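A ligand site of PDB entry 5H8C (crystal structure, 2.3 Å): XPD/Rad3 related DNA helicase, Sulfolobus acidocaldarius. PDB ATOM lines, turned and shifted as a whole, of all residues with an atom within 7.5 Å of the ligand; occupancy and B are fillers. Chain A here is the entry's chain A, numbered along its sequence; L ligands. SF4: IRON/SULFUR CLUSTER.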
ATOM      1  N   LYS A  84     -15.084 -18.100  32.666  1.00  0.00           N
ATOM      2  CA  LYS A  84     -14.465 -17.189  31.704  1.00  0.00           C
ATOM      3  C   LYS A  84     -15.495 -16.298  30.974  1.00  0.00           C
ATOM      4  O   LYS A  84     -15.268 -15.106  30.867  1.00  0.00           O
ATOM      5  CB  LYS A  84     -13.585 -17.947  30.687  1.00  0.00           C
ATOM      6  CG  LYS A  84     -12.352 -18.605  31.285  1.00  0.00           C
ATOM      7  CD  LYS A  84     -11.659 -19.506  30.278  1.00  0.00           C
ATOM      8  CE  LYS A  84     -10.195 -19.738  30.621  1.00  0.00           C
ATOM      9  NZ  LYS A  84      -9.517 -20.671  29.681  1.00  0.00           N
ATOM     10  N   PRO A  85     -16.624 -16.867  30.492  1.00  0.00           N
ATOM     11  CA  PRO A  85     -17.653 -16.039  29.844  1.00  0.00           C
ATOM     12  C   PRO A  85     -18.209 -14.867  30.660  1.00  0.00           C
ATOM     13  O   PRO A  85     -18.680 -13.897  30.072  1.00  0.00           O
ATOM     14  CB  PRO A  85     -18.793 -17.035  29.591  1.00  0.00           C
ATOM     15  CG  PRO A  85     -18.132 -18.362  29.495  1.00  0.00           C
ATOM     16  CD  PRO A  85     -16.934 -18.309  30.385  1.00  0.00           C
ATOM     17  N   SER A  87     -16.243 -13.425  33.176  1.00  0.00           N
ATOM     18  CA  SER A  87     -15.083 -12.641  33.618  1.00  0.00           C
ATOM     19  C   SER A  87     -14.090 -12.166  32.525  1.00  0.00           C
ATOM     20  O   SER A  87     -13.418 -11.170  32.746  1.00  0.00           O
ATOM     21  CB  SER A  87     -14.339 -13.379  34.712  1.00  0.00           C
ATOM     22  OG  SER A  87     -14.006 -14.666  34.291  1.00  0.00           O
ATOM     23  N   CYS A  88     -14.002 -12.846  31.375  1.00  0.00           N
ATOM     24  CA  CYS A  88     -13.154 -12.396  30.247  1.00  0.00           C
ATOM     25  C   CYS A  88     -13.482 -10.977  29.790  1.00  0.00           C
ATOM     26  O   CYS A  88     -14.662 -10.610  29.688  1.00  0.00           O
ATOM     27  CB  CYS A  88     -13.330 -13.305  29.017  1.00  0.00           C
ATOM     28  SG  CYS A  88     -12.318 -12.777  27.586  1.00  0.00           S
ATOM     29  N   LEU A  89     -12.459 -10.191  29.470  1.00  0.00           N
ATOM     30  CA  LEU A  89     -12.661  -8.809  29.010  1.00  0.00           C
ATOM     31  C   LEU A  89     -13.480  -8.686  27.709  1.00  0.00           C
ATOM     32  O   LEU A  89     -14.190  -7.696  27.521  1.00  0.00           O
ATOM     33  CB  LEU A  89     -11.324  -8.074  28.856  1.00  0.00           C
ATOM     34  CG  LEU A  89     -10.467  -7.837  30.114  1.00  0.00           C
ATOM     35  CD1 LEU A  89      -9.201  -7.065  29.742  1.00  0.00           C
ATOM     36  CD2 LEU A  89     -11.250  -7.087  31.179  1.00  0.00           C
ATOM     37  N   TYR A  90     -13.382  -9.706  26.839  1.00  0.00           N
ATOM     38  CA  TYR A  90     -13.890  -9.640  25.465  1.00  0.00           C
ATOM     39  C   TYR A  90     -15.140 -10.501  25.211  1.00  0.00           C
ATOM     40  O   TYR A  90     -15.660 -10.490  24.102  1.00  0.00           O
ATOM     41  CB  TYR A  90     -12.784 -10.104  24.514  1.00  0.00           C
ATOM     42  CG  TYR A  90     -11.451  -9.483  24.822  1.00  0.00           C
ATOM     43  CD1 TYR A  90     -11.237  -8.109  24.657  1.00  0.00           C
ATOM     44  CD2 TYR A  90     -10.403 -10.254  25.321  1.00  0.00           C
ATOM     45  CE1 TYR A  90     -10.021  -7.537  24.959  1.00  0.00           C
ATOM     46  CE2 TYR A  90      -9.176  -9.683  25.614  1.00  0.00           C
ATOM     47  CZ  TYR A  90      -8.989  -8.331  25.440  1.00  0.00           C
ATOM     48  OH  TYR A  90      -7.781  -7.782  25.745  1.00  0.00           O
ATOM     49  N   ALA A  91     -15.608 -11.234  26.216  1.00  0.00           N
ATOM     50  CA  ALA A  91     -16.715 -12.179  26.035  1.00  0.00           C
ATOM     51  C   ALA A  91     -18.065 -11.471  25.876  1.00  0.00           C
ATOM     52  O   ALA A  91     -18.340 -10.491  26.565  1.00  0.00           O
ATOM     53  CB  ALA A  91     -16.770 -13.161  27.201  1.00  0.00           C
ATOM     54  N   ASP A  99     -14.588 -21.361  23.856  1.00  0.00           N
ATOM     55  CA  ASP A  99     -14.479 -20.322  22.811  1.00  0.00           C
ATOM     56  C   ASP A  99     -13.541 -19.186  23.246  1.00  0.00           C
ATOM     57  O   ASP A  99     -12.998 -18.468  22.391  1.00  0.00           O
ATOM     58  CB  ASP A  99     -15.855 -19.706  22.456  1.00  0.00           C
ATOM     59  CG  ASP A  99     -16.888 -20.740  21.984  1.00  0.00           C
ATOM     60  OD1 ASP A  99     -16.531 -21.898  21.621  1.00  0.00           O
ATOM     61  OD2 ASP A  99     -18.079 -20.370  21.984  1.00  0.00           O
ATOM     62  N   ILE A 100     -13.338 -19.015  24.555  1.00  0.00           N
ATOM     63  CA  ILE A 100     -12.544 -17.905  25.062  1.00  0.00           C
ATOM     64  C   ILE A 100     -11.099 -18.183  24.653  1.00  0.00           C
ATOM     65  O   ILE A 100     -10.548 -19.222  25.005  1.00  0.00           O
ATOM     66  CB  ILE A 100     -12.680 -17.710  26.579  1.00  0.00           C
ATOM     67  CG1 ILE A 100     -14.163 -17.506  26.984  1.00  0.00           C
ATOM     68  CG2 ILE A 100     -11.851 -16.528  27.039  1.00  0.00           C
ATOM     69  CD1 ILE A 100     -14.854 -16.314  26.363  1.00  0.00           C
ATOM     70  N   PRO A 101     -10.493 -17.264  23.875  1.00  0.00           N
ATOM     71  CA  PRO A 101      -9.225 -17.581  23.177  1.00  0.00           C
ATOM     72  C   PRO A 101      -7.962 -17.229  23.989  1.00  0.00           C
ATOM     73  O   PRO A 101      -7.093 -16.508  23.496  1.00  0.00           O
ATOM     74  CB  PRO A 101      -9.340 -16.728  21.920  1.00  0.00           C
ATOM     75  CG  PRO A 101     -10.047 -15.504  22.398  1.00  0.00           C
ATOM     76  CD  PRO A 101     -11.000 -15.936  23.466  1.00  0.00           C
ATOM     77  N   CYS A 102      -7.864 -17.748  25.217  1.00  0.00           N
ATOM     78  CA  CYS A 102      -6.758 -17.406  26.106  1.00  0.00           C
ATOM     79  C   CYS A 102      -5.375 -17.835  25.542  1.00  0.00           C
ATOM     80  O   CYS A 102      -4.382 -17.124  25.703  1.00  0.00           O
ATOM     81  CB  CYS A 102      -6.984 -18.001  27.506  1.00  0.00           C
ATOM     82  SG  CYS A 102      -8.513 -17.448  28.294  1.00  0.00           S
ATOM     83  N   LYS A 103      -5.351 -18.970  24.852  1.00  0.00           N
ATOM     84  CA  LYS A 103      -4.169 -19.432  24.097  1.00  0.00           C
ATOM     85  C   LYS A 103      -3.458 -18.310  23.320  1.00  0.00           C
ATOM     86  O   LYS A 103      -2.233 -18.304  23.259  1.00  0.00           O
ATOM     87  CB  LYS A 103      -4.592 -20.533  23.112  1.00  0.00           C
ATOM     88  CG  LYS A 103      -3.452 -21.340  22.532  1.00  0.00           C
ATOM     89  CD  LYS A 103      -3.977 -22.549  21.759  1.00  0.00           C
ATOM     90  CE  LYS A 103      -2.831 -23.437  21.294  1.00  0.00           C
ATOM     91  NZ  LYS A 103      -1.994 -22.809  20.230  1.00  0.00           N
ATOM     92  N   TYR A 104      -4.215 -17.360  22.766  1.00  0.00           N
ATOM     93  CA  TYR A 104      -3.691 -16.267  21.935  1.00  0.00           C
ATOM     94  C   TYR A 104      -3.624 -14.879  22.601  1.00  0.00           C
ATOM     95  O   TYR A 104      -3.159 -13.910  21.982  1.00  0.00           O
ATOM     96  CB  TYR A 104      -4.529 -16.167  20.660  1.00  0.00           C
ATOM     97  CG  TYR A 104      -4.721 -17.497  19.972  1.00  0.00           C
ATOM     98  CD1 TYR A 104      -3.687 -18.081  19.228  1.00  0.00           C
ATOM     99  CD2 TYR A 104      -5.925 -18.197  20.085  1.00  0.00           C
ATOM    100  CE1 TYR A 104      -3.856 -19.314  18.615  1.00  0.00           C
ATOM    101  CE2 TYR A 104      -6.100 -19.434  19.464  1.00  0.00           C
ATOM    102  CZ  TYR A 104      -5.062 -19.991  18.732  1.00  0.00           C
ATOM    103  OH  TYR A 104      -5.244 -21.209  18.123  1.00  0.00           O
ATOM    104  N   CYS A 105      -4.069 -14.780  23.851  1.00  0.00           N
ATOM    105  CA  CYS A 105      -4.251 -13.496  24.534  1.00  0.00           C
ATOM    106  C   CYS A 105      -3.017 -13.109  25.326  1.00  0.00           C
ATOM    107  O   CYS A 105      -2.438 -13.944  26.026  1.00  0.00           O
ATOM    108  CB  CYS A 105      -5.447 -13.597  25.499  1.00  0.00           C
ATOM    109  SG  CYS A 105      -5.886 -12.068  26.345  1.00  0.00           S
ATOM    110  N   GLU A 106      -2.645 -11.839  25.257  1.00  0.00           N
ATOM    111  CA  GLU A 106      -1.489 -11.304  26.005  1.00  0.00           C
ATOM    112  C   GLU A 106      -1.697 -11.242  27.517  1.00  0.00           C
ATOM    113  O   GLU A 106      -0.724 -11.178  28.284  1.00  0.00           O
ATOM    114  CB  GLU A 106      -1.108  -9.905  25.491  1.00  0.00           C
ATOM    115  CG  GLU A 106      -0.600  -9.899  24.061  1.00  0.00           C
ATOM    116  CD  GLU A 106      -0.064  -8.536  23.642  1.00  0.00           C
ATOM    117  OE1 GLU A 106      -0.779  -7.526  23.869  1.00  0.00           O
ATOM    118  OE2 GLU A 106       1.057  -8.471  23.066  1.00  0.00           O
ATOM    119  N   LEU A 107      -2.952 -11.270  27.966  1.00  0.00           N
ATOM    120  CA  LEU A 107      -3.256 -11.135  29.399  1.00  0.00           C
ATOM    121  C   LEU A 107      -3.245 -12.456  30.162  1.00  0.00           C
ATOM    122  O   LEU A 107      -3.335 -12.425  31.376  1.00  0.00           O
ATOM    123  CB  LEU A 107      -4.583 -10.389  29.585  1.00  0.00           C
ATOM    124  CG  LEU A 107      -4.631  -9.019  28.871  1.00  0.00           C
ATOM    125  CD1 LEU A 107      -6.012  -8.391  28.908  1.00  0.00           C
ATOM    126  CD2 LEU A 107      -3.586  -8.074  29.454  1.00  0.00           C
ATOM    127  N   LYS A 108      -3.121 -13.598  29.476  1.00  0.00           N
ATOM    128  CA  LYS A 108      -3.233 -14.929  30.125  1.00  0.00           C
ATOM    129  C   LYS A 108      -2.344 -15.084  31.370  1.00  0.00           C
ATOM    130  O   LYS A 108      -2.784 -15.655  32.374  1.00  0.00           O
ATOM    131  CB  LYS A 108      -2.921 -16.052  29.130  1.00  0.00           C
ATOM    132  CG  LYS A 108      -3.135 -17.462  29.678  1.00  0.00           C
ATOM    133  CD  LYS A 108      -2.678 -18.526  28.689  1.00  0.00           C
ATOM    134  CE  LYS A 108      -2.489 -19.889  29.342  1.00  0.00           C
ATOM    135  NZ  LYS A 108      -3.728 -20.386  30.004  1.00  0.00           N
ATOM    136  N   GLY A 109      -1.109 -14.582  31.281  1.00  0.00           N
ATOM    137  CA  GLY A 109      -0.169 -14.590  32.405  1.00  0.00           C
ATOM    138  C   GLY A 109      -0.042 -13.242  33.110  1.00  0.00           C
ATOM    139  O   GLY A 109       1.065 -12.869  33.535  1.00  0.00           O
ATOM    140  N   SER A 110      -1.159 -12.528  33.250  1.00  0.00           N
ATOM    141  CA  SER A 110      -1.199 -11.206  33.855  1.00  0.00           C
ATOM    142  C   SER A 110      -2.258 -11.209  34.965  1.00  0.00           C
ATOM    143  O   SER A 110      -3.441 -10.994  34.704  1.00  0.00           O
ATOM    144  CB  SER A 110      -1.473 -10.136  32.792  1.00  0.00           C
ATOM    145  OG  SER A 110      -1.357  -8.836  33.336  1.00  0.00           O
ATOM    146  N   PHE A 136      -4.791  -6.532  32.934  1.00  0.00           N
ATOM    147  CA  PHE A 136      -4.713  -7.844  33.585  1.00  0.00           C
ATOM    148  C   PHE A 136      -5.986  -8.630  33.276  1.00  0.00           C
ATOM    149  O   PHE A 136      -6.990  -8.046  32.853  1.00  0.00           O
ATOM    150  CB  PHE A 136      -4.468  -7.718  35.099  1.00  0.00           C
ATOM    151  CG  PHE A 136      -5.545  -6.967  35.842  1.00  0.00           C
ATOM    152  CD1 PHE A 136      -6.687  -7.620  36.292  1.00  0.00           C
ATOM    153  CD2 PHE A 136      -5.407  -5.603  36.123  1.00  0.00           C
ATOM    154  CE1 PHE A 136      -7.672  -6.936  36.978  1.00  0.00           C
ATOM    155  CE2 PHE A 136      -6.392  -4.919  36.809  1.00  0.00           C
ATOM    156  CZ  PHE A 136      -7.533  -5.593  37.240  1.00  0.00           C
ATOM    157  N   CYS A 137      -5.910  -9.938  33.450  1.00  0.00           N
ATOM    158  CA  CYS A 137      -7.054 -10.811  33.185  1.00  0.00           C
ATOM    159  C   CYS A 137      -7.884 -10.994  34.450  1.00  0.00           C
ATOM    160  O   CYS A 137      -7.372 -11.492  35.459  1.00  0.00           O
ATOM    161  CB  CYS A 137      -6.587 -12.171  32.717  1.00  0.00           C
ATOM    162  SG  CYS A 137      -7.960 -13.263  32.299  1.00  0.00           S
ATOM    163  N   PRO A 138      -9.176 -10.632  34.400  1.00  0.00           N
ATOM    164  CA  PRO A 138     -10.066 -10.864  35.545  1.00  0.00           C
ATOM    165  C   PRO A 138     -10.189 -12.324  35.975  1.00  0.00           C
ATOM    166  O   PRO A 138     -10.100 -12.625  37.181  1.00  0.00           O
ATOM    167  CB  PRO A 138     -11.416 -10.341  35.061  1.00  0.00           C
ATOM    168  CG  PRO A 138     -11.096  -9.388  33.967  1.00  0.00           C
ATOM    169  CD  PRO A 138      -9.869  -9.931  33.308  1.00  0.00           C
ATOM    170  N   TYR A 139     -10.451 -13.202  35.004  1.00  0.00           N
ATOM    171  CA  TYR A 139     -10.536 -14.642  35.232  1.00  0.00           C
ATOM    172  C   TYR A 139      -9.329 -15.200  35.982  1.00  0.00           C
ATOM    173  O   TYR A 139      -9.501 -15.783  37.062  1.00  0.00           O
ATOM    174  CB  TYR A 139     -10.756 -15.418  33.923  1.00  0.00           C
ATOM    175  CG  TYR A 139     -10.905 -16.907  34.169  1.00  0.00           C
ATOM    176  CD1 TYR A 139     -12.071 -17.426  34.755  1.00  0.00           C
ATOM    177  CD2 TYR A 139      -9.857 -17.797  33.893  1.00  0.00           C
ATOM    178  CE1 TYR A 139     -12.211 -18.785  35.004  1.00  0.00           C
ATOM    179  CE2 TYR A 139      -9.985 -19.159  34.147  1.00  0.00           C
ATOM    180  CZ  TYR A 139     -11.162 -19.653  34.702  1.00  0.00           C
ATOM    181  OH  TYR A 139     -11.296 -21.008  34.958  1.00  0.00           O
ATOM    182  N   TYR A 140      -8.126 -15.018  35.451  1.00  0.00           N
ATOM    183  CA  TYR A 140      -6.933 -15.611  36.079  1.00  0.00           C
ATOM    184  C   TYR A 140      -6.620 -14.932  37.397  1.00  0.00           C
ATOM    185  O   TYR A 140      -6.021 -15.538  38.277  1.00  0.00           O
ATOM    186  CB  TYR A 140      -5.725 -15.654  35.129  1.00  0.00           C
ATOM    187  CG  TYR A 140      -5.941 -16.692  34.043  1.00  0.00           C
ATOM    188  CD1 TYR A 140      -5.901 -18.057  34.355  1.00  0.00           C
ATOM    189  CD2 TYR A 140      -6.271 -16.321  32.741  1.00  0.00           C
ATOM    190  CE1 TYR A 140      -6.160 -19.015  33.390  1.00  0.00           C
ATOM    191  CE2 TYR A 140      -6.523 -17.284  31.761  1.00  0.00           C
ATOM    192  CZ  TYR A 140      -6.462 -18.623  32.097  1.00  0.00           C
ATOM    193  OH  TYR A 140      -6.714 -19.580  31.153  1.00  0.00           O
ATOM    194  N   LEU A 263     -10.493 -12.780  19.001  1.00  0.00           N
ATOM    195  CA  LEU A 263      -9.570 -12.034  19.868  1.00  0.00           C
ATOM    196  C   LEU A 263      -8.999 -10.795  19.205  1.00  0.00           C
ATOM    197  O   LEU A 263      -8.692  -9.812  19.889  1.00  0.00           O
ATOM    198  CB  LEU A 263      -8.407 -12.912  20.336  1.00  0.00           C
ATOM    199  CG  LEU A 263      -7.414 -12.256  21.309  1.00  0.00           C
ATOM    200  CD1 LEU A 263      -8.080 -11.955  22.646  1.00  0.00           C
ATOM    201  CD2 LEU A 263      -6.167 -13.106  21.493  1.00  0.00           C
ATOM    202  N   VAL A 268     -15.839 -11.911  21.610  1.00  0.00           N
ATOM    203  CA  VAL A 268     -15.953 -13.376  21.532  1.00  0.00           C
ATOM    204  C   VAL A 268     -17.429 -13.779  21.567  1.00  0.00           C
ATOM    205  O   VAL A 268     -18.104 -13.543  22.559  1.00  0.00           O
ATOM    206  CB  VAL A 268     -15.200 -14.065  22.678  1.00  0.00           C
ATOM    207  CG1 VAL A 268     -15.215 -15.580  22.503  1.00  0.00           C
ATOM    208  CG2 VAL A 268     -13.763 -13.552  22.762  1.00  0.00           C
HETATM  209 FE1  SF4 L   1      -8.516 -13.355  30.081  1.00  0.00          FE
HETATM  210 FE2  SF4 L   1      -8.497 -15.184  28.390  1.00  0.00          FE
HETATM  211 FE3  SF4 L   1     -10.178 -13.258  28.205  1.00  0.00          FE
HETATM  212 FE4  SF4 L   1      -7.666 -12.905  27.688  1.00  0.00          FE
HETATM  213  S1  SF4 L   1      -9.019 -14.146  26.669  1.00  0.00           S
HETATM  214  S2  SF4 L   1      -8.942 -11.710  28.867  1.00  0.00           S
HETATM  215  S3  SF4 L   1      -6.781 -14.170  29.124  1.00  0.00           S
HETATM  216  S4  SF4 L   1     -10.084 -14.734  29.719  1.00  0.00           S
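FE2 of the ligand is bound by SG of Cys 102 (2.3 Å).
SG of Cys 88 binds FE3 of the ligand, at 2.3 Å.
FE1 of the ligand is bound by SG of Cys 137 (2.3 Å).
FE4 of the ligand is bound by SG of Cys 105.
N of Lys 108 lies close to S3 of the ligand (3.7 Å).
The side-chain sulfur (SG) of Cys 102 sits close to the side-chain amino group (NZ) of Lys 84.
The side-chain sulfur (SG) of Cys 88 sits close to the backbone NH (N) of Tyr 90 (3.3 Å).
The backbone NH of Tyr 140 lies close to the side-chain sulfur of Cys 137.
SG of Cys 137 lies close to N of Tyr 139 (3.7 Å).
The backbone carbonyl oxygen (O) of Ser 110 is in hydrogen-bond range of the backbone NH (N) of Cys 137 (3.0 Å).
SG of Cys 105 lies close to N of Leu 107.
The side-chain hydroxyl (OH) of Tyr 140 lies within hydrogen-bond range of the side-chain amino group (NZ) of Lys 108, 3.3 Å away.
The backbone NH (N) of Val 268 is in hydrogen-bond range of the backbone carbonyl oxygen (O) of Tyr 90, 2.9 Å away.
Leu 89 touches the ligand.
CE2 of Tyr 90 touches S2 of the ligand, 3.8 Å away.
Ile 100 touches the ligand.
Hydrophobic or aromatic side chains that line the ligand: Tyr 90 and Ile 100.
Of the 26 residues printed, 8 come within 4 Å of the ligand.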
